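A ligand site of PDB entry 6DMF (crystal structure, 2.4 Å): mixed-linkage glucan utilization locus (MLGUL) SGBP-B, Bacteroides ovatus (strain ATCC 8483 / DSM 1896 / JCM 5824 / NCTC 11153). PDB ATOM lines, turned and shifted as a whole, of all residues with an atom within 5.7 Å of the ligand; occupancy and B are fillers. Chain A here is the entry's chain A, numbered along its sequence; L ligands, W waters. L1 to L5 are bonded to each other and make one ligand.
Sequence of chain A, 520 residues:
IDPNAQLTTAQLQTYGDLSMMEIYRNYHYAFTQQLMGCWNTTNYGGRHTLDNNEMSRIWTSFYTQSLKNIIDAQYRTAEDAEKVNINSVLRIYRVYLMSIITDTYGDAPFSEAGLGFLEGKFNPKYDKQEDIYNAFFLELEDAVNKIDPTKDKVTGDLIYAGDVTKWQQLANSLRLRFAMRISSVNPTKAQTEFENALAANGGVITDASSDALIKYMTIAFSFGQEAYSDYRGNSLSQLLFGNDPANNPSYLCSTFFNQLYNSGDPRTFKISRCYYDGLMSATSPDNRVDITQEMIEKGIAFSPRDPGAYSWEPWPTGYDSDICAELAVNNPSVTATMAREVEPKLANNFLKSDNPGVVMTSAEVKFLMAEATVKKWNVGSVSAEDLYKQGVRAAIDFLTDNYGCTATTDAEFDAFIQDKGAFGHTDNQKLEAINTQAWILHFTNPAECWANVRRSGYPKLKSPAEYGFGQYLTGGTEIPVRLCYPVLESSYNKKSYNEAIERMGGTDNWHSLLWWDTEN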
ATOM      1  N   LEU A  18       7.977  -7.044 -24.101  1.00  0.00           N
ATOM      2  CA  LEU A  18       7.795  -8.513 -24.092  1.00  0.00           C
ATOM      3  C   LEU A  18       7.985  -9.064 -25.517  1.00  0.00           C
ATOM      4  O   LEU A  18       8.497 -10.161 -25.679  1.00  0.00           O
ATOM      5  CB  LEU A  18       6.395  -8.873 -23.568  1.00  0.00           C
ATOM      6  CG  LEU A  18       6.292 -10.123 -22.690  1.00  0.00           C
ATOM      7  CD1 LEU A  18       4.909 -10.757 -22.817  1.00  0.00           C
ATOM      8  CD2 LEU A  18       7.362 -11.164 -22.985  1.00  0.00           C
ATOM      9  N   SER A  19       7.533  -8.303 -26.510  1.00  0.00           N
ATOM     10  CA  SER A  19       7.691  -8.677 -27.923  1.00  0.00           C
ATOM     11  C   SER A  19       9.181  -8.809 -28.276  1.00  0.00           C
ATOM     12  O   SER A  19       9.585  -9.816 -28.873  1.00  0.00           O
ATOM     13  CB  SER A  19       6.999  -7.690 -28.833  1.00  0.00           C
ATOM     14  OG  SER A  19       7.330  -7.936 -30.191  1.00  0.00           O
ATOM     15  N   GLU A  22      11.863 -11.773 -27.056  1.00  0.00           N
ATOM     16  CA  GLU A  22      11.788 -13.067 -27.777  1.00  0.00           C
ATOM     17  C   GLU A  22      13.093 -13.320 -28.547  1.00  0.00           C
ATOM     18  O   GLU A  22      13.570 -14.465 -28.622  1.00  0.00           O
ATOM     19  CB  GLU A  22      10.594 -13.113 -28.749  1.00  0.00           C
ATOM     20  CG  GLU A  22       9.250 -13.316 -28.075  1.00  0.00           C
ATOM     21  CD  GLU A  22       8.819 -14.754 -27.805  1.00  0.00           C
ATOM     22  OE1 GLU A  22       9.331 -15.681 -28.467  1.00  0.00           O
ATOM     23  OE2 GLU A  22       7.962 -14.948 -26.924  1.00  0.00           O
ATOM     24  N   ARG A  25      15.997 -14.890 -26.264  1.00  0.00           N
ATOM     25  CA  ARG A  25      15.766 -16.290 -25.893  1.00  0.00           C
ATOM     26  C   ARG A  25      15.841 -17.195 -27.136  1.00  0.00           C
ATOM     27  O   ARG A  25      16.294 -18.343 -27.043  1.00  0.00           O
ATOM     28  CB  ARG A  25      14.407 -16.465 -25.192  1.00  0.00           C
ATOM     29  CG  ARG A  25      14.074 -17.929 -24.925  1.00  0.00           C
ATOM     30  CD  ARG A  25      12.863 -18.153 -24.040  1.00  0.00           C
ATOM     31  NE  ARG A  25      11.618 -18.158 -24.794  1.00  0.00           N
ATOM     32  CZ  ARG A  25      10.475 -18.683 -24.357  1.00  0.00           C
ATOM     33  NH1 ARG A  25      10.442 -19.303 -23.192  1.00  0.00           N
ATOM     34  NH2 ARG A  25       9.384 -18.590 -25.093  1.00  0.00           N
ATOM     35  N   TRP A  39      12.410 -25.322 -26.165  1.00  0.00           N
ATOM     36  CA  TRP A  39      12.026 -25.517 -27.547  1.00  0.00           C
ATOM     37  C   TRP A  39      12.441 -24.317 -28.397  1.00  0.00           C
ATOM     38  O   TRP A  39      12.962 -24.487 -29.500  1.00  0.00           O
ATOM     39  CB  TRP A  39      10.523 -25.795 -27.705  1.00  0.00           C
ATOM     40  CG  TRP A  39      10.173 -25.843 -29.153  1.00  0.00           C
ATOM     41  CD1 TRP A  39      10.319 -26.905 -30.000  1.00  0.00           C
ATOM     42  CD2 TRP A  39       9.741 -24.744 -29.972  1.00  0.00           C
ATOM     43  NE1 TRP A  39       9.958 -26.560 -31.275  1.00  0.00           N
ATOM     44  CE2 TRP A  39       9.600 -25.238 -31.295  1.00  0.00           C
ATOM     45  CE3 TRP A  39       9.431 -23.394 -29.720  1.00  0.00           C
ATOM     46  CZ2 TRP A  39       9.164 -24.429 -32.349  1.00  0.00           C
ATOM     47  CZ3 TRP A  39       8.998 -22.603 -30.761  1.00  0.00           C
ATOM     48  CH2 TRP A  39       8.869 -23.117 -32.060  1.00  0.00           C
ATOM     49  N   ASN A  40      12.180 -23.097 -27.884  1.00  0.00           N
ATOM     50  CA  ASN A  40      12.372 -21.862 -28.671  1.00  0.00           C
ATOM     51  C   ASN A  40      13.867 -21.680 -28.962  1.00  0.00           C
ATOM     52  O   ASN A  40      14.268 -21.432 -30.103  1.00  0.00           O
ATOM     53  CB  ASN A  40      11.795 -20.628 -27.972  1.00  0.00           C
ATOM     54  CG  ASN A  40      10.374 -20.794 -27.497  1.00  0.00           C
ATOM     55  OD1 ASN A  40      10.090 -21.682 -26.691  1.00  0.00           O
ATOM     56  ND2 ASN A  40       9.477 -19.936 -27.969  1.00  0.00           N
ATOM     57  N   GLU A  54      11.205 -13.293 -36.690  1.00  0.00           N
ATOM     58  CA  GLU A  54      11.859 -13.488 -35.401  1.00  0.00           C
ATOM     59  C   GLU A  54      13.160 -12.673 -35.322  1.00  0.00           C
ATOM     60  O   GLU A  54      13.548 -12.257 -34.249  1.00  0.00           O
ATOM     61  CB  GLU A  54      12.160 -14.959 -35.145  1.00  0.00           C
ATOM     62  CG  GLU A  54      10.944 -15.777 -34.765  1.00  0.00           C
ATOM     63  CD  GLU A  54      10.131 -15.191 -33.621  1.00  0.00           C
ATOM     64  OE1 GLU A  54      10.741 -14.627 -32.689  1.00  0.00           O
ATOM     65  OE2 GLU A  54       8.902 -15.268 -33.684  1.00  0.00           O
ATOM     66  N   ARG A  57      13.008  -8.202 -34.611  1.00  0.00           N
ATOM     67  CA  ARG A  57      12.277  -7.685 -33.456  1.00  0.00           C
ATOM     68  C   ARG A  57      12.967  -6.436 -32.887  1.00  0.00           C
ATOM     69  O   ARG A  57      12.287  -5.476 -32.525  1.00  0.00           O
ATOM     70  CB  ARG A  57      12.100  -8.794 -32.416  1.00  0.00           C
ATOM     71  CG  ARG A  57      11.312  -9.984 -32.938  1.00  0.00           C
ATOM     72  CD  ARG A  57      10.888 -10.949 -31.841  1.00  0.00           C
ATOM     73  NE  ARG A  57       9.498 -10.716 -31.471  1.00  0.00           N
ATOM     74  CZ  ARG A  57       8.493 -11.543 -31.726  1.00  0.00           C
ATOM     75  NH1 ARG A  57       8.731 -12.770 -32.138  1.00  0.00           N
ATOM     76  NH2 ARG A  57       7.254 -11.129 -31.542  1.00  0.00           N
ATOM     77  N   GLN A 225      -2.717  -9.758 -24.124  1.00  0.00           N
ATOM     78  CA  GLN A 225      -2.423  -8.712 -25.106  1.00  0.00           C
ATOM     79  C   GLN A 225      -2.039  -7.398 -24.399  1.00  0.00           C
ATOM     80  O   GLN A 225      -1.183  -6.657 -24.901  1.00  0.00           O
ATOM     81  CB  GLN A 225      -3.609  -8.493 -26.047  1.00  0.00           C
ATOM     82  CG  GLN A 225      -3.201  -7.898 -27.392  1.00  0.00           C
ATOM     83  CD  GLN A 225      -4.354  -7.253 -28.125  1.00  0.00           C
ATOM     84  OE1 GLN A 225      -5.507  -7.659 -28.003  1.00  0.00           O
ATOM     85  NE2 GLN A 225      -4.039  -6.229 -28.904  1.00  0.00           N
ATOM     86  N   TYR A 228       1.750  -6.588 -23.522  1.00  0.00           N
ATOM     87  CA  TYR A 228       2.699  -6.230 -24.572  1.00  0.00           C
ATOM     88  C   TYR A 228       2.915  -4.704 -24.646  1.00  0.00           C
ATOM     89  O   TYR A 228       3.868  -4.251 -25.272  1.00  0.00           O
ATOM     90  CB  TYR A 228       2.276  -6.852 -25.905  1.00  0.00           C
ATOM     91  CG  TYR A 228       2.623  -8.313 -26.003  1.00  0.00           C
ATOM     92  CD1 TYR A 228       3.859  -8.728 -26.492  1.00  0.00           C
ATOM     93  CD2 TYR A 228       1.751  -9.292 -25.549  1.00  0.00           C
ATOM     94  CE1 TYR A 228       4.198 -10.074 -26.554  1.00  0.00           C
ATOM     95  CE2 TYR A 228       2.083 -10.640 -25.605  1.00  0.00           C
ATOM     96  CZ  TYR A 228       3.311 -11.030 -26.111  1.00  0.00           C
ATOM     97  OH  TYR A 228       3.640 -12.351 -26.160  1.00  0.00           O
ATOM     98  N   ASN A 243       6.445 -18.718 -21.255  1.00  0.00           N
ATOM     99  CA  ASN A 243       5.035 -18.818 -21.608  1.00  0.00           C
ATOM    100  C   ASN A 243       4.544 -20.242 -21.359  1.00  0.00           C
ATOM    101  O   ASN A 243       3.369 -20.462 -21.110  1.00  0.00           O
ATOM    102  CB  ASN A 243       4.772 -18.414 -23.067  1.00  0.00           C
ATOM    103  CG  ASN A 243       5.757 -19.031 -24.054  1.00  0.00           C
ATOM    104  OD1 ASN A 243       6.906 -18.613 -24.142  1.00  0.00           O
ATOM    105  ND2 ASN A 243       5.298 -20.012 -24.824  1.00  0.00           N
ATOM    106  N   ASP A 244       5.478 -21.209 -21.432  1.00  0.00           N
ATOM    107  CA  ASP A 244       5.244 -22.642 -21.243  1.00  0.00           C
ATOM    108  C   ASP A 244       6.254 -23.162 -20.227  1.00  0.00           C
ATOM    109  O   ASP A 244       7.058 -24.047 -20.550  1.00  0.00           O
ATOM    110  CB  ASP A 244       5.331 -23.366 -22.584  1.00  0.00           C
ATOM    111  CG  ASP A 244       4.983 -24.848 -22.559  1.00  0.00           C
ATOM    112  OD1 ASP A 244       4.243 -25.259 -21.647  1.00  0.00           O
ATOM    113  OD2 ASP A 244       5.468 -25.572 -23.442  1.00  0.00           O
ATOM    114  N   ASN A 247       7.183 -27.257 -19.286  1.00  0.00           N
ATOM    115  CA  ASN A 247       7.703 -28.097 -20.387  1.00  0.00           C
ATOM    116  C   ASN A 247       8.963 -27.480 -20.989  1.00  0.00           C
ATOM    117  O   ASN A 247       9.881 -28.208 -21.389  1.00  0.00           O
ATOM    118  CB  ASN A 247       6.656 -28.294 -21.482  1.00  0.00           C
ATOM    119  CG  ASN A 247       5.360 -28.885 -20.965  1.00  0.00           C
ATOM    120  OD1 ASN A 247       5.374 -29.855 -20.210  1.00  0.00           O
ATOM    121  ND2 ASN A 247       4.239 -28.297 -21.362  1.00  0.00           N
ATOM    122  N   ASN A 248       9.003 -26.144 -21.080  1.00  0.00           N
ATOM    123  CA  ASN A 248      10.069 -25.427 -21.773  1.00  0.00           C
ATOM    124  C   ASN A 248      10.598 -24.289 -20.902  1.00  0.00           C
ATOM    125  O   ASN A 248      10.398 -23.120 -21.232  1.00  0.00           O
ATOM    126  CB  ASN A 248       9.578 -24.971 -23.153  1.00  0.00           C
ATOM    127  CG  ASN A 248       9.412 -26.143 -24.091  1.00  0.00           C
ATOM    128  OD1 ASN A 248      10.395 -26.739 -24.522  1.00  0.00           O
ATOM    129  ND2 ASN A 248       8.164 -26.488 -24.400  1.00  0.00           N
ATOM    130  N   TRP A 312      14.510 -33.125 -24.405  1.00  0.00           N
ATOM    131  CA  TRP A 312      13.932 -34.467 -24.469  1.00  0.00           C
ATOM    132  C   TRP A 312      14.831 -35.457 -25.246  1.00  0.00           C
ATOM    133  O   TRP A 312      14.598 -36.656 -25.163  1.00  0.00           O
ATOM    134  CB  TRP A 312      12.502 -34.423 -25.040  1.00  0.00           C
ATOM    135  CG  TRP A 312      12.362 -33.644 -26.312  1.00  0.00           C
ATOM    136  CD1 TRP A 312      12.634 -34.078 -27.569  1.00  0.00           C
ATOM    137  CD2 TRP A 312      11.908 -32.282 -26.439  1.00  0.00           C
ATOM    138  NE1 TRP A 312      12.381 -33.082 -28.483  1.00  0.00           N
ATOM    139  CE2 TRP A 312      11.931 -31.973 -27.821  1.00  0.00           C
ATOM    140  CE3 TRP A 312      11.489 -31.299 -25.537  1.00  0.00           C
ATOM    141  CZ2 TRP A 312      11.557 -30.720 -28.306  1.00  0.00           C
ATOM    142  CZ3 TRP A 312      11.116 -30.060 -26.026  1.00  0.00           C
ATOM    143  CH2 TRP A 312      11.152 -29.784 -27.387  1.00  0.00           C
ATOM    144  N   ARG A 340      14.355 -35.364 -16.734  1.00  0.00           N
ATOM    145  CA  ARG A 340      14.783 -34.104 -17.360  1.00  0.00           C
ATOM    146  C   ARG A 340      15.226 -33.095 -16.283  1.00  0.00           C
ATOM    147  O   ARG A 340      15.871 -32.083 -16.614  1.00  0.00           O
ATOM    148  CB  ARG A 340      13.659 -33.530 -18.233  1.00  0.00           C
ATOM    149  CG  ARG A 340      13.466 -34.283 -19.541  1.00  0.00           C
ATOM    150  CD  ARG A 340      12.596 -33.533 -20.538  1.00  0.00           C
ATOM    151  NE  ARG A 340      11.184 -33.593 -20.211  1.00  0.00           N
ATOM    152  CZ  ARG A 340      10.227 -32.996 -20.912  1.00  0.00           C
ATOM    153  NH1 ARG A 340      10.526 -32.252 -21.971  1.00  0.00           N
ATOM    154  NH2 ARG A 340       8.954 -33.144 -20.559  1.00  0.00           N
HETATM  155  C1  LIG L   1       3.461  -8.920 -30.939  1.00  0.00           C
HETATM  156  C2  LIG L   1       3.229 -10.408 -31.153  1.00  0.00           C
HETATM  157  C3  LIG L   1       2.157 -10.922 -30.204  1.00  0.00           C
HETATM  158  C4  LIG L   1       0.907 -10.028 -30.195  1.00  0.00           C
HETATM  159  C5  LIG L   1      -0.120 -10.448 -29.136  1.00  0.00           C
HETATM  160  C6  LIG L   1       2.134  -8.176 -31.004  1.00  0.00           C
HETATM  161  O1  LIG L   1       2.368  -6.786 -30.810  1.00  0.00           O
HETATM  162  O2  LIG L   1       4.344  -8.437 -31.958  1.00  0.00           O
HETATM  163  O3  LIG L   1       4.464 -11.106 -30.937  1.00  0.00           O
HETATM  164  O4  LIG L   1       1.813 -12.247 -30.629  1.00  0.00           O
HETATM  165  O5  LIG L   1       1.277  -8.661 -29.970  1.00  0.00           O
HETATM  166  O6  LIG L   1      -1.438 -10.038 -29.521  1.00  0.00           O
HETATM  167  C1  LG2 L   2       1.554 -14.550 -29.997  1.00  0.00           C
HETATM  168  C2  LG2 L   2       2.109 -15.630 -29.064  1.00  0.00           C
HETATM  169  C3  LG2 L   2       3.563 -15.881 -29.427  1.00  0.00           C
HETATM  170  C4  LG2 L   2       4.306 -14.545 -29.307  1.00  0.00           C
HETATM  171  C5  LG2 L   2       5.775 -14.673 -29.651  1.00  0.00           C
HETATM  172  C6  LG2 L   2       2.365 -13.282 -29.816  1.00  0.00           C
HETATM  173  O1  LG2 L   2       0.161 -14.299 -29.723  1.00  0.00           O
HETATM  174  O2  LG2 L   2       1.368 -16.849 -29.155  1.00  0.00           O
HETATM  175  O3  LG2 L   2       4.125 -16.866 -28.548  1.00  0.00           O
HETATM  176  O4  LG2 L   2       3.720 -13.567 -30.168  1.00  0.00           O
HETATM  177  O5  LG2 L   2       6.337 -13.360 -29.486  1.00  0.00           O
HETATM  178  C1  LG3 L   3       5.578 -18.792 -28.271  1.00  0.00           C
HETATM  179  C2  LG3 L   3       6.039 -20.137 -28.845  1.00  0.00           C
HETATM  180  C3  LG3 L   3       4.939 -20.880 -29.621  1.00  0.00           C
HETATM  181  C4  LG3 L   3       4.314 -19.891 -30.595  1.00  0.00           C
HETATM  182  C5  LG3 L   3       3.254 -20.499 -31.502  1.00  0.00           C
HETATM  183  C6  LG3 L   3       4.719 -17.987 -29.249  1.00  0.00           C
HETATM  184  O1  LG3 L   3       6.729 -18.000 -27.911  1.00  0.00           O
HETATM  185  O2  LG3 L   3       6.517 -20.938 -27.750  1.00  0.00           O
HETATM  186  O3  LG3 L   3       5.471 -22.011 -30.338  1.00  0.00           O
HETATM  187  O4  LG3 L   3       3.735 -18.835 -29.835  1.00  0.00           O
HETATM  188  O5  LG3 L   3       2.164 -20.966 -30.707  1.00  0.00           O
HETATM  189  C1  LG4 L   4       5.609 -24.405 -30.736  1.00  0.00           C
HETATM  190  C2  LG4 L   4       5.417 -25.808 -30.147  1.00  0.00           C
HETATM  191  C3  LG4 L   4       6.192 -25.933 -28.826  1.00  0.00           C
HETATM  192  C4  LG4 L   4       5.747 -24.780 -27.908  1.00  0.00           C
HETATM  193  C5  LG4 L   4       6.450 -24.797 -26.552  1.00  0.00           C
HETATM  194  C6  LG4 L   4       5.232 -23.311 -29.737  1.00  0.00           C
HETATM  195  O1  LG4 L   4       4.848 -24.243 -31.941  1.00  0.00           O
HETATM  196  O2  LG4 L   4       5.849 -26.833 -31.050  1.00  0.00           O
HETATM  197  O3  LG4 L   4       5.906 -27.205 -28.208  1.00  0.00           O
HETATM  198  O4  LG4 L   4       5.969 -23.513 -28.528  1.00  0.00           O
HETATM  199  O5  LG4 L   4       6.079 -23.625 -25.815  1.00  0.00           O
HETATM  200  C1  LG5 L   5       6.672 -29.237 -27.214  1.00  0.00           C
HETATM  201  C2  LG5 L   5       7.552 -30.487 -27.349  1.00  0.00           C
HETATM  202  C3  LG5 L   5       7.312 -31.142 -28.712  1.00  0.00           C
HETATM  203  C4  LG5 L   5       7.638 -30.090 -29.784  1.00  0.00           C
HETATM  204  C5  LG5 L   5       7.442 -30.643 -31.184  1.00  0.00           C
HETATM  205  C6  LG5 L   5       6.901 -28.247 -28.366  1.00  0.00           C
HETATM  206  O1  LG5 L   5       6.933 -28.546 -25.976  1.00  0.00           O
HETATM  207  O2  LG5 L   5       7.330 -31.446 -26.310  1.00  0.00           O
HETATM  208  O3  LG5 L   5       8.085 -32.350 -28.852  1.00  0.00           O
HETATM  209  O4  LG5 L   5       6.824 -28.913 -29.625  1.00  0.00           O
HETATM  210  O5  LG5 L   5       6.306 -30.017 -31.785  1.00  0.00           O
HETATM  211  O   HOH W   1       8.152 -22.009 -25.056  1.00  0.00           O
HETATM  212  O   HOH W   2       8.472 -34.051 -26.612  1.00  0.00           O
HETATM  213  O   HOH W   3       4.807 -27.667 -24.523  1.00  0.00           O
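An oxygen (O5) of LG2 L2 sits close to the side-chain carboxylate (OE2) of Glu 22 (3.4 Å). The side-chain amide nitrogen of Asn 248 sits at hydrogen-bond distance from an oxygen (O1) of LG5 L5, at 2.9 Å. NH2 of Arg 57 is in hydrogen-bond range of O3 of LIG L1 (2.9 Å). The side-chain carboxylate (OD2) of Asp 244 sits at hydrogen-bond distance from an oxygen (O5) of LG4 L4, at 3.1 Å. An oxygen (O2) of LG3 L3 is in hydrogen-bond range of the side-chain amide nitrogen (ND2) of Asn 40, 3.1 Å away. ND2 of Asn 243 sits at hydrogen-bond distance from O2 of LG3 L3 (3.3 Å).
The guanidinium group (NE) of Arg 57 lies within hydrogen-bond range of the backbone carbonyl oxygen (O) of Ser 19, 2.8 Å away. The guanidinium group (NH2) of Arg 25 sits close to the side-chain amide nitrogen (ND2) of Asn 40, 3.2 Å away. The side-chain carboxylate of Asp 244 sits at hydrogen-bond distance from the side-chain amide nitrogen of Asn 247, 3.1 Å away. OD1 of Asn 248 is in hydrogen-bond range of N of Trp 39, at 3.0 Å. The guanidinium group (NH2) of Arg 25 is in hydrogen-bond range of the side-chain amide oxygen (OD1) of Asn 243 (2.7 Å). OD2 of Asp 244 is in hydrogen-bond range of ND2 of Asn 248 (3.0 Å). The guanidinium group (NH1) of Arg 57 lies within salt-bridge range of the side-chain carboxylate (OE1) of Glu 54 (2.8 Å).
Residues that only touch the ligand: Gln 225 (3.5 Å), Ser 19 (3.5 Å), Trp 39 (3.6 Å), Trp 312 (3.7 Å), Tyr 228 (3.9 Å) and Arg 25 (3.9 Å). Within 4 Å of the ligand: Ser 19, Glu 22, Arg 25, Trp 39, Asn 40, Arg 57, Gln 225, Tyr 228, Asn 243, Asp 244, Asn 248 and Trp 312.
Water W3 lies within hydrogen-bond range of OD2 of Asp 244 (2.4 Å), O1 of LG5 L5 (2.7 Å) and ND2 of Asn 247 (3.3 Å). Water W1 lies within hydrogen-bond range of the side-chain amide oxygen of Asn 40 (2.6 Å), an oxygen (O5) of LG4 L4 (2.7 Å) and the side-chain amide nitrogen of Asn 243 (3.5 Å).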
